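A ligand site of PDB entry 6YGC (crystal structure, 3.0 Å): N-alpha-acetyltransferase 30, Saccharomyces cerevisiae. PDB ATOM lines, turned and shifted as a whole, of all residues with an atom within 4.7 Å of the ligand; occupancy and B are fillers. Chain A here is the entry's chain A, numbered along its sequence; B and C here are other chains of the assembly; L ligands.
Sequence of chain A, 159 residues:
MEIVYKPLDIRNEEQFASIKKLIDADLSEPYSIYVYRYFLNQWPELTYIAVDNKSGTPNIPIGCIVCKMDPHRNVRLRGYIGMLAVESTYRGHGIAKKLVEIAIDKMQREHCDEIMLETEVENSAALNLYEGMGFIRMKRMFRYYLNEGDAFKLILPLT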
ATOM      1  N   ASP A  26      15.097   6.480 -17.960  1.00  0.00           N
ATOM      2  CA  ASP A  26      15.552   5.253 -18.610  1.00  0.00           C
ATOM      3  C   ASP A  26      14.431   4.483 -19.316  1.00  0.00           C
ATOM      4  O   ASP A  26      14.678   3.362 -19.778  1.00  0.00           O
ATOM      5  CB  ASP A  26      16.230   4.346 -17.580  1.00  0.00           C
ATOM      6  CG  ASP A  26      17.506   4.958 -17.013  1.00  0.00           C
ATOM      7  OD1 ASP A  26      18.384   5.355 -17.809  1.00  0.00           O
ATOM      8  OD2 ASP A  26      17.616   5.056 -15.774  1.00  0.00           O
ATOM      9  N   LEU A  84      11.912  -1.606 -13.672  1.00  0.00           N
ATOM     10  CA  LEU A  84      13.205  -1.894 -13.050  1.00  0.00           C
ATOM     11  C   LEU A  84      14.232  -0.980 -13.700  1.00  0.00           C
ATOM     12  O   LEU A  84      14.385  -0.997 -14.928  1.00  0.00           O
ATOM     13  CB  LEU A  84      13.608  -3.360 -13.239  1.00  0.00           C
ATOM     14  CG  LEU A  84      15.075  -3.683 -12.933  1.00  0.00           C
ATOM     15  CD1 LEU A  84      15.350  -3.629 -11.441  1.00  0.00           C
ATOM     16  CD2 LEU A  84      15.456  -5.041 -13.513  1.00  0.00           C
ATOM     17  N   ALA A  85      14.947  -0.203 -12.886  1.00  0.00           N
ATOM     18  CA  ALA A  85      15.940   0.729 -13.406  1.00  0.00           C
ATOM     19  C   ALA A  85      16.995   0.981 -12.337  1.00  0.00           C
ATOM     20  O   ALA A  85      16.711   1.019 -11.143  1.00  0.00           O
ATOM     21  CB  ALA A  85      15.314   2.045 -13.848  1.00  0.00           C
ATOM     22  N   VAL A  86      18.241   1.162 -12.797  1.00  0.00           N
ATOM     23  CA  VAL A  86      19.379   1.459 -11.939  1.00  0.00           C
ATOM     24  C   VAL A  86      20.084   2.681 -12.508  1.00  0.00           C
ATOM     25  O   VAL A  86      20.148   2.854 -13.731  1.00  0.00           O
ATOM     26  CB  VAL A  86      20.345   0.259 -11.840  1.00  0.00           C
ATOM     27  CG1 VAL A  86      21.501   0.575 -10.901  1.00  0.00           C
ATOM     28  CG2 VAL A  86      19.611  -0.981 -11.369  1.00  0.00           C
ATOM     29  N   TYR A  90      25.857   3.465 -11.470  1.00  0.00           N
ATOM     30  CA  TYR A  90      25.863   2.358 -10.524  1.00  0.00           C
ATOM     31  C   TYR A  90      25.665   0.999 -11.199  1.00  0.00           C
ATOM     32  O   TYR A  90      25.551  -0.014 -10.504  1.00  0.00           O
ATOM     33  CB  TYR A  90      24.776   2.556  -9.463  1.00  0.00           C
ATOM     34  CG  TYR A  90      25.169   3.477  -8.334  1.00  0.00           C
ATOM     35  CD1 TYR A  90      25.900   3.008  -7.256  1.00  0.00           C
ATOM     36  CD2 TYR A  90      24.808   4.816  -8.349  1.00  0.00           C
ATOM     37  CE1 TYR A  90      26.269   3.841  -6.217  1.00  0.00           C
ATOM     38  CE2 TYR A  90      25.164   5.658  -7.314  1.00  0.00           C
ATOM     39  CZ  TYR A  90      25.886   5.171  -6.255  1.00  0.00           C
ATOM     40  OH  TYR A  90      26.250   6.003  -5.224  1.00  0.00           O
ATOM     41  N   ARG A  91      25.643   0.953 -12.528  1.00  0.00           N
ATOM     42  CA  ARG A  91      25.391  -0.295 -13.218  1.00  0.00           C
ATOM     43  C   ARG A  91      26.623  -1.193 -13.206  1.00  0.00           C
ATOM     44  O   ARG A  91      27.759  -0.722 -13.087  1.00  0.00           O
ATOM     45  CB  ARG A  91      24.937  -0.040 -14.657  1.00  0.00           C
ATOM     46  CG  ARG A  91      23.642   0.739 -14.751  1.00  0.00           C
ATOM     47  CD  ARG A  91      23.273   1.055 -16.198  1.00  0.00           C
ATOM     48  NE  ARG A  91      22.187   2.024 -16.274  1.00  0.00           N
ATOM     49  CZ  ARG A  91      21.746   2.574 -17.399  1.00  0.00           C
ATOM     50  NH1 ARG A  91      22.313   2.246 -18.553  1.00  0.00           N
ATOM     51  NH2 ARG A  91      20.761   3.451 -17.370  1.00  0.00           N
ATOM     52  N   GLY A  92      26.387  -2.491 -13.343  1.00  0.00           N
ATOM     53  CA  GLY A  92      27.459  -3.469 -13.316  1.00  0.00           C
ATOM     54  C   GLY A  92      27.885  -3.913 -11.935  1.00  0.00           C
ATOM     55  O   GLY A  92      28.908  -4.603 -11.822  1.00  0.00           O
ATOM     56  N   HIS A  93      27.147  -3.544 -10.894  1.00  0.00           N
ATOM     57  CA  HIS A  93      27.501  -3.878  -9.518  1.00  0.00           C
ATOM     58  C   HIS A  93      26.559  -4.882  -8.879  1.00  0.00           C
ATOM     59  O   HIS A  93      26.593  -5.064  -7.662  1.00  0.00           O
ATOM     60  CB  HIS A  93      27.558  -2.613  -8.659  1.00  0.00           C
ATOM     61  CG  HIS A  93      28.724  -1.725  -8.954  1.00  0.00           C
ATOM     62  ND1 HIS A  93      29.348  -0.961  -7.991  1.00  0.00           N
ATOM     63  CD2 HIS A  93      29.384  -1.483 -10.112  1.00  0.00           C
ATOM     64  CE1 HIS A  93      30.341  -0.289  -8.537  1.00  0.00           C
ATOM     65  NE2 HIS A  93      30.378  -0.586  -9.823  1.00  0.00           N
ATOM     66  N   GLY A  94      25.718  -5.549  -9.672  1.00  0.00           N
ATOM     67  CA  GLY A  94      24.793  -6.502  -9.109  1.00  0.00           C
ATOM     68  C   GLY A  94      23.603  -5.897  -8.393  1.00  0.00           C
ATOM     69  O   GLY A  94      22.898  -6.622  -7.681  1.00  0.00           O
ATOM     70  N   ILE A  95      23.360  -4.604  -8.573  1.00  0.00           N
ATOM     71  CA  ILE A  95      22.290  -3.930  -7.839  1.00  0.00           C
ATOM     72  C   ILE A  95      20.925  -4.394  -8.335  1.00  0.00           C
ATOM     73  O   ILE A  95      20.056  -4.780  -7.543  1.00  0.00           O
ATOM     74  CB  ILE A  95      22.446  -2.407  -7.961  1.00  0.00           C
ATOM     75  CG1 ILE A  95      23.733  -1.957  -7.268  1.00  0.00           C
ATOM     76  CG2 ILE A  95      21.227  -1.700  -7.364  1.00  0.00           C
ATOM     77  CD1 ILE A  95      24.014  -0.483  -7.410  1.00  0.00           C
ATOM     78  N   ALA A  96      20.706  -4.330  -9.651  1.00  0.00           N
ATOM     79  CA  ALA A  96      19.421  -4.743 -10.209  1.00  0.00           C
ATOM     80  C   ALA A  96      19.124  -6.209  -9.901  1.00  0.00           C
ATOM     81  O   ALA A  96      17.984  -6.567  -9.611  1.00  0.00           O
ATOM     82  CB  ALA A  96      19.392  -4.506 -11.721  1.00  0.00           C
ATOM     83  N   LYS A  97      20.163  -7.056  -9.957  1.00  0.00           N
ATOM     84  CA  LYS A  97      19.987  -8.482  -9.676  1.00  0.00           C
ATOM     85  C   LYS A  97      19.416  -8.699  -8.281  1.00  0.00           C
ATOM     86  O   LYS A  97      18.458  -9.464  -8.104  1.00  0.00           O
ATOM     87  CB  LYS A  97      21.324  -9.197  -9.828  1.00  0.00           C
ATOM     88  CG  LYS A  97      21.266 -10.709  -9.711  1.00  0.00           C
ATOM     89  CD  LYS A  97      22.652 -11.303  -9.897  1.00  0.00           C
ATOM     90  CE  LYS A  97      22.618 -12.811 -10.018  1.00  0.00           C
ATOM     91  NZ  LYS A  97      23.966 -13.362 -10.341  1.00  0.00           N
ATOM     92  N   GLU A 118       7.473  -8.401 -19.476  1.00  0.00           N
ATOM     93  CA  GLU A 118       7.731  -8.205 -20.889  1.00  0.00           C
ATOM     94  C   GLU A 118       8.975  -7.339 -21.055  1.00  0.00           C
ATOM     95  O   GLU A 118       9.225  -6.443 -20.246  1.00  0.00           O
ATOM     96  CB  GLU A 118       6.544  -7.544 -21.604  1.00  0.00           C
ATOM     97  CG  GLU A 118       5.224  -8.270 -21.452  1.00  0.00           C
ATOM     98  CD  GLU A 118       4.333  -7.641 -20.396  1.00  0.00           C
ATOM     99  OE1 GLU A 118       4.791  -6.702 -19.705  1.00  0.00           O
ATOM    100  OE2 GLU A 118       3.178  -8.086 -20.245  1.00  0.00           O
ATOM    101  N   THR A 119       9.744  -7.618 -22.099  1.00  0.00           N
ATOM    102  CA  THR A 119      10.947  -6.841 -22.370  1.00  0.00           C
ATOM    103  C   THR A 119      11.276  -6.933 -23.847  1.00  0.00           C
ATOM    104  O   THR A 119      10.795  -7.821 -24.559  1.00  0.00           O
ATOM    105  CB  THR A 119      12.140  -7.333 -21.531  1.00  0.00           C
ATOM    106  OG1 THR A 119      13.209  -6.399 -21.640  1.00  0.00           O
ATOM    107  CG2 THR A 119      12.610  -8.684 -22.022  1.00  0.00           C
ATOM    108  N   GLU A 120      12.100  -5.993 -24.302  1.00  0.00           N
ATOM    109  CA  GLU A 120      12.461  -5.946 -25.715  1.00  0.00           C
ATOM    110  C   GLU A 120      13.390  -7.098 -26.079  1.00  0.00           C
ATOM    111  O   GLU A 120      14.153  -7.602 -25.244  1.00  0.00           O
ATOM    112  CB  GLU A 120      13.151  -4.619 -26.049  1.00  0.00           C
ATOM    113  CG  GLU A 120      12.389  -3.377 -25.645  1.00  0.00           C
ATOM    114  CD  GLU A 120      12.822  -2.831 -24.294  1.00  0.00           C
ATOM    115  OE1 GLU A 120      12.850  -3.609 -23.320  1.00  0.00           O
ATOM    116  OE2 GLU A 120      13.151  -1.631 -24.219  1.00  0.00           O
ATOM    117  N   ASN A 123      16.988  -5.898 -25.667  1.00  0.00           N
ATOM    118  CA  ASN A 123      17.506  -5.601 -24.331  1.00  0.00           C
ATOM    119  C   ASN A 123      18.280  -6.818 -23.840  1.00  0.00           C
ATOM    120  O   ASN A 123      17.791  -7.644 -23.061  1.00  0.00           O
ATOM    121  CB  ASN A 123      16.368  -5.230 -23.387  1.00  0.00           C
ATOM    122  CG  ASN A 123      16.848  -4.522 -22.137  1.00  0.00           C
ATOM    123  OD1 ASN A 123      17.990  -4.707 -21.717  1.00  0.00           O
ATOM    124  ND2 ASN A 123      15.982  -3.714 -21.552  1.00  0.00           N
ATOM    125  N   SER A 124      19.526  -6.927 -24.305  1.00  0.00           N
ATOM    126  CA  SER A 124      20.371  -8.053 -23.916  1.00  0.00           C
ATOM    127  C   SER A 124      20.725  -8.009 -22.444  1.00  0.00           C
ATOM    128  O   SER A 124      20.888  -9.050 -21.803  1.00  0.00           O
ATOM    129  CB  SER A 124      21.643  -8.074 -24.766  1.00  0.00           C
ATOM    130  OG  SER A 124      21.339  -8.230 -26.142  1.00  0.00           O
ATOM    131  N   ALA A 125      20.837  -6.798 -21.873  1.00  0.00           N
ATOM    132  CA  ALA A 125      21.164  -6.684 -20.453  1.00  0.00           C
ATOM    133  C   ALA A 125      20.046  -7.232 -19.581  1.00  0.00           C
ATOM    134  O   ALA A 125      20.311  -7.920 -18.581  1.00  0.00           O
ATOM    135  CB  ALA A 125      21.447  -5.219 -20.113  1.00  0.00           C
ATOM    136  N   ALA A 126      18.793  -6.948 -19.930  1.00  0.00           N
ATOM    137  CA  ALA A 126      17.668  -7.415 -19.132  1.00  0.00           C
ATOM    138  C   ALA A 126      17.396  -8.902 -19.366  1.00  0.00           C
ATOM    139  O   ALA A 126      17.030  -9.620 -18.434  1.00  0.00           O
ATOM    140  CB  ALA A 126      16.423  -6.592 -19.432  1.00  0.00           C
ATOM    141  N   ASN A 128      19.578 -11.333 -20.186  1.00  0.00           N
ATOM    142  CA  ASN A 128      20.564 -12.144 -19.471  1.00  0.00           C
ATOM    143  C   ASN A 128      20.302 -12.131 -17.973  1.00  0.00           C
ATOM    144  O   ASN A 128      20.564 -13.133 -17.292  1.00  0.00           O
ATOM    145  CB  ASN A 128      21.977 -11.635 -19.753  1.00  0.00           C
ATOM    146  CG  ASN A 128      22.379 -11.838 -21.202  1.00  0.00           C
ATOM    147  OD1 ASN A 128      21.535 -11.904 -22.096  1.00  0.00           O
ATOM    148  ND2 ASN A 128      23.682 -11.931 -21.450  1.00  0.00           N
ATOM    149  N   LEU A 129      19.774 -11.032 -17.445  1.00  0.00           N
ATOM    150  CA  LEU A 129      19.484 -10.948 -16.022  1.00  0.00           C
ATOM    151  C   LEU A 129      18.360 -11.898 -15.626  1.00  0.00           C
ATOM    152  O   LEU A 129      18.491 -12.665 -14.671  1.00  0.00           O
ATOM    153  CB  LEU A 129      19.128  -9.505 -15.655  1.00  0.00           C
ATOM    154  CG  LEU A 129      18.524  -9.222 -14.269  1.00  0.00           C
ATOM    155  CD1 LEU A 129      19.403  -9.790 -13.168  1.00  0.00           C
ATOM    156  CD2 LEU A 129      18.326  -7.726 -14.074  1.00  0.00           C
ATOM    157  N   TYR A 130      17.246 -11.867 -16.367  1.00  0.00           N
ATOM    158  CA  TYR A 130      16.090 -12.677 -15.986  1.00  0.00           C
ATOM    159  C   TYR A 130      16.303 -14.140 -16.346  1.00  0.00           C
ATOM    160  O   TYR A 130      16.093 -15.026 -15.509  1.00  0.00           O
ATOM    161  CB  TYR A 130      14.827 -12.137 -16.653  1.00  0.00           C
ATOM    162  CG  TYR A 130      14.406 -10.777 -16.153  1.00  0.00           C
ATOM    163  CD1 TYR A 130      14.177 -10.562 -14.804  1.00  0.00           C
ATOM    164  CD2 TYR A 130      14.222  -9.721 -17.030  1.00  0.00           C
ATOM    165  CE1 TYR A 130      13.796  -9.321 -14.338  1.00  0.00           C
ATOM    166  CE2 TYR A 130      13.831  -8.480 -16.582  1.00  0.00           C
ATOM    167  CZ  TYR A 130      13.611  -8.285 -15.238  1.00  0.00           C
ATOM    168  OH  TYR A 130      13.225  -7.044 -14.781  1.00  0.00           O
ATOM    169  N   MET B   1       9.648  -4.142 -19.637  1.00  0.00           N
ATOM    170  CA  MET B   1       8.997  -3.047 -18.911  1.00  0.00           C
ATOM    171  C   MET B   1       7.484  -3.107 -19.076  1.00  0.00           C
ATOM    172  O   MET B   1       6.947  -4.079 -19.592  1.00  0.00           O
ATOM    173  CB  MET B   1       9.538  -1.697 -19.381  1.00  0.00           C
ATOM    174  CG  MET B   1       9.567  -1.529 -20.891  1.00  0.00           C
ATOM    175  SD  MET B   1      10.232   0.061 -21.398  1.00  0.00           S
ATOM    176  CE  MET B   1      11.883  -0.028 -20.688  1.00  0.00           C
ATOM    177  N   ARG C 733      32.378  -8.116 -20.677  1.00  0.00           N
ATOM    178  CA  ARG C 733      32.090  -6.796 -21.226  1.00  0.00           C
ATOM    179  C   ARG C 733      33.078  -5.753 -20.728  1.00  0.00           C
ATOM    180  O   ARG C 733      32.696  -4.651 -20.332  1.00  0.00           O
ATOM    181  CB  ARG C 733      30.658  -6.386 -20.873  1.00  0.00           C
ATOM    182  CG  ARG C 733      29.623  -7.442 -21.201  1.00  0.00           C
ATOM    183  CD  ARG C 733      28.265  -7.065 -20.661  1.00  0.00           C
ATOM    184  NE  ARG C 733      28.275  -6.861 -19.222  1.00  0.00           N
ATOM    185  CZ  ARG C 733      28.052  -7.828 -18.324  1.00  0.00           C
ATOM    186  NH1 ARG C 733      27.812  -9.061 -18.728  1.00  0.00           N
ATOM    187  NH2 ARG C 733      28.086  -7.541 -17.031  1.00  0.00           N
HETATM  188  N1  LIG L   1      25.021  -6.575 -21.003  1.00  0.00           N
HETATM  189  C1  LIG L   1      24.680  -7.896 -20.996  1.00  0.00           C
HETATM  190  N2  LIG L   1      24.241  -8.479 -19.833  1.00  0.00           N
HETATM  191  C2  LIG L   1      24.147  -7.739 -18.691  1.00  0.00           C
HETATM  192  C3  LIG L   1      24.483  -6.448 -18.708  1.00  0.00           C
HETATM  193  C4  LIG L   1      24.931  -5.855 -19.898  1.00  0.00           C
HETATM  194  N3  LIG L   1      25.345  -4.520 -20.156  1.00  0.00           N
HETATM  195  N4  LIG L   1      24.297  -5.951 -17.466  1.00  0.00           N
HETATM  196  C5  LIG L   1      23.853  -6.936 -16.691  1.00  0.00           C
HETATM  197  N5  LIG L   1      23.752  -8.043 -17.435  1.00  0.00           N
HETATM  198  C6  LIG L   1      23.318  -9.361 -17.041  1.00  0.00           C
HETATM  199  C7  LIG L   1      24.356 -10.134 -16.792  1.00  0.00           C
HETATM  200  O1  LIG L   1      24.016 -11.489 -17.089  1.00  0.00           O
HETATM  201  C8  LIG L   1      24.599  -9.971 -15.271  1.00  0.00           C
HETATM  202  O2  LIG L   1      25.199 -11.049 -14.766  1.00  0.00           O
HETATM  203  P1  LIG L   1      26.894 -11.115 -14.799  1.00  0.00           P
HETATM  204  O3  LIG L   1      27.454  -9.865 -14.144  1.00  0.00           O
HETATM  205  O4  LIG L   1      27.386 -12.368 -14.027  1.00  0.00           O
HETATM  206  O5  LIG L   1      27.367 -11.188 -16.238  1.00  0.00           O
HETATM  207  C9  LIG L   1      23.153  -9.824 -14.690  1.00  0.00           C
HETATM  208  O6  LIG L   1      22.442  -9.279 -15.641  1.00  0.00           O
HETATM  209  C10 LIG L   1      23.158  -8.917 -13.461  1.00  0.00           C
HETATM  210  O7  LIG L   1      23.423  -7.599 -13.857  1.00  0.00           O
HETATM  211  P2  LIG L   1      23.364  -6.400 -12.703  1.00  0.00           P
HETATM  212  O8  LIG L   1      24.747  -5.851 -12.474  1.00  0.00           O
HETATM  213  O9  LIG L   1      22.845  -6.984 -11.431  1.00  0.00           O
HETATM  214  O10 LIG L   1      22.326  -5.203 -13.182  1.00  0.00           O
HETATM  215  P3  LIG L   1      22.753  -3.568 -13.386  1.00  0.00           P
HETATM  216  O11 LIG L   1      22.863  -2.892 -12.024  1.00  0.00           O
HETATM  217  O12 LIG L   1      24.071  -3.472 -14.122  1.00  0.00           O
HETATM  218  O13 LIG L   1      21.554  -2.854 -14.274  1.00  0.00           O
HETATM  219  C11 LIG L   1      19.780  -2.909 -15.902  1.00  0.00           C
HETATM  220  C12 LIG L   1      20.984  -3.637 -15.309  1.00  0.00           C
HETATM  221  C13 LIG L   1      18.989  -3.876 -16.714  1.00  0.00           C
HETATM  222  C14 LIG L   1      18.912  -2.381 -14.781  1.00  0.00           C
HETATM  223  C15 LIG L   1      20.280  -1.741 -16.782  1.00  0.00           C
HETATM  224  O14 LIG L   1      20.816  -2.249 -17.935  1.00  0.00           O
HETATM  225  C16 LIG L   1      19.119  -0.767 -17.134  1.00  0.00           C
HETATM  226  O15 LIG L   1      18.986   0.282 -16.518  1.00  0.00           O
HETATM  227  N6  LIG L   1      18.161  -1.109 -18.255  1.00  0.00           N
HETATM  228  C17 LIG L   1      17.032  -0.155 -18.612  1.00  0.00           C
HETATM  229  C18 LIG L   1      15.773  -0.532 -17.810  1.00  0.00           C
HETATM  230  C19 LIG L   1      15.178  -1.844 -18.358  1.00  0.00           C
HETATM  231  O16 LIG L   1      15.016  -1.973 -19.526  1.00  0.00           O
HETATM  232  N7  LIG L   1      14.844  -2.891 -17.460  1.00  0.00           N
HETATM  233  C20 LIG L   1      14.290  -4.153 -17.950  1.00  0.00           C
HETATM  234  C21 LIG L   1      12.808  -3.948 -18.419  1.00  0.00           C
HETATM  235  S1  LIG L   1      11.684  -4.901 -17.303  1.00  0.00           S
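N of Ala 126 sits at hydrogen-bond distance from OD1 of Asn 123 (3.0 Å).
The backbone NH of Met 1 of chain B sits at hydrogen-bond distance from the backbone carbonyl oxygen of Glu 118 (2.4 Å).
The backbone carbonyl oxygen (O) of Ser 124 sits close to the side-chain amide oxygen (OD1) of Asn 128.
NE of Arg 91 sits at hydrogen-bond distance from O of Val 86 (3.4 Å).
NH2 of Arg 91 lies within salt-bridge range of OD1 of Asp 26 (3.1 Å).
Val 86 touches the ligand.
Arg 91 touches the ligand (C to O12, 3.5 Å).
His 93 touches the ligand.
Ile 95 touches the ligand (N to O9, 3.8 Å).
CB of Ala 96 touches O10 of the ligand, 3.4 Å away.
Ser 124 touches the ligand (O to N2, 3.9 Å).
Ala 125 touches the ligand (CB to C4, 3.5 Å).
Ala 126 touches the ligand.
Asn 128 touches the ligand.
Leu 129 touches the ligand.
18 residues have an atom within 4 Å of the ligand: Leu 84, Val 86, Arg 91, Gly 92, His 93, Gly 94, Ile 95, Ala 96, Lys 97, Asn 123, Ser 124, Ala 125, Ala 126, Asn 128, Leu 129, Tyr 130, Met 1 of chain B and Arg 733 of chain C.
O12 of the ligand sits at hydrogen-bond distance from N of Gly 92 (2.6 Å).
An oxygen (O16) of the ligand lies within hydrogen-bond range of the side-chain amide nitrogen (ND2) of Asn 123, at 2.8 Å.
An oxygen (O8) of the ligand sits at hydrogen-bond distance from the backbone NH (N) of Gly 94, at 3.0 Å.
N of Lys 97 sits at hydrogen-bond distance from O9 of the ligand (3.1 Å).
N of Met 1 of chain B sits close to S1 of the ligand (3.2 Å).
N7 of the ligand is in hydrogen-bond range of O of Leu 84, 3.2 Å away.
The guanidinium group (NH1) of Arg 733 of chain C is in salt-bridge range of an oxygen (O5) of the ligand, at 3.3 Å.
S1 of the ligand sits close to OH of Tyr 130 (3.7 Å).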
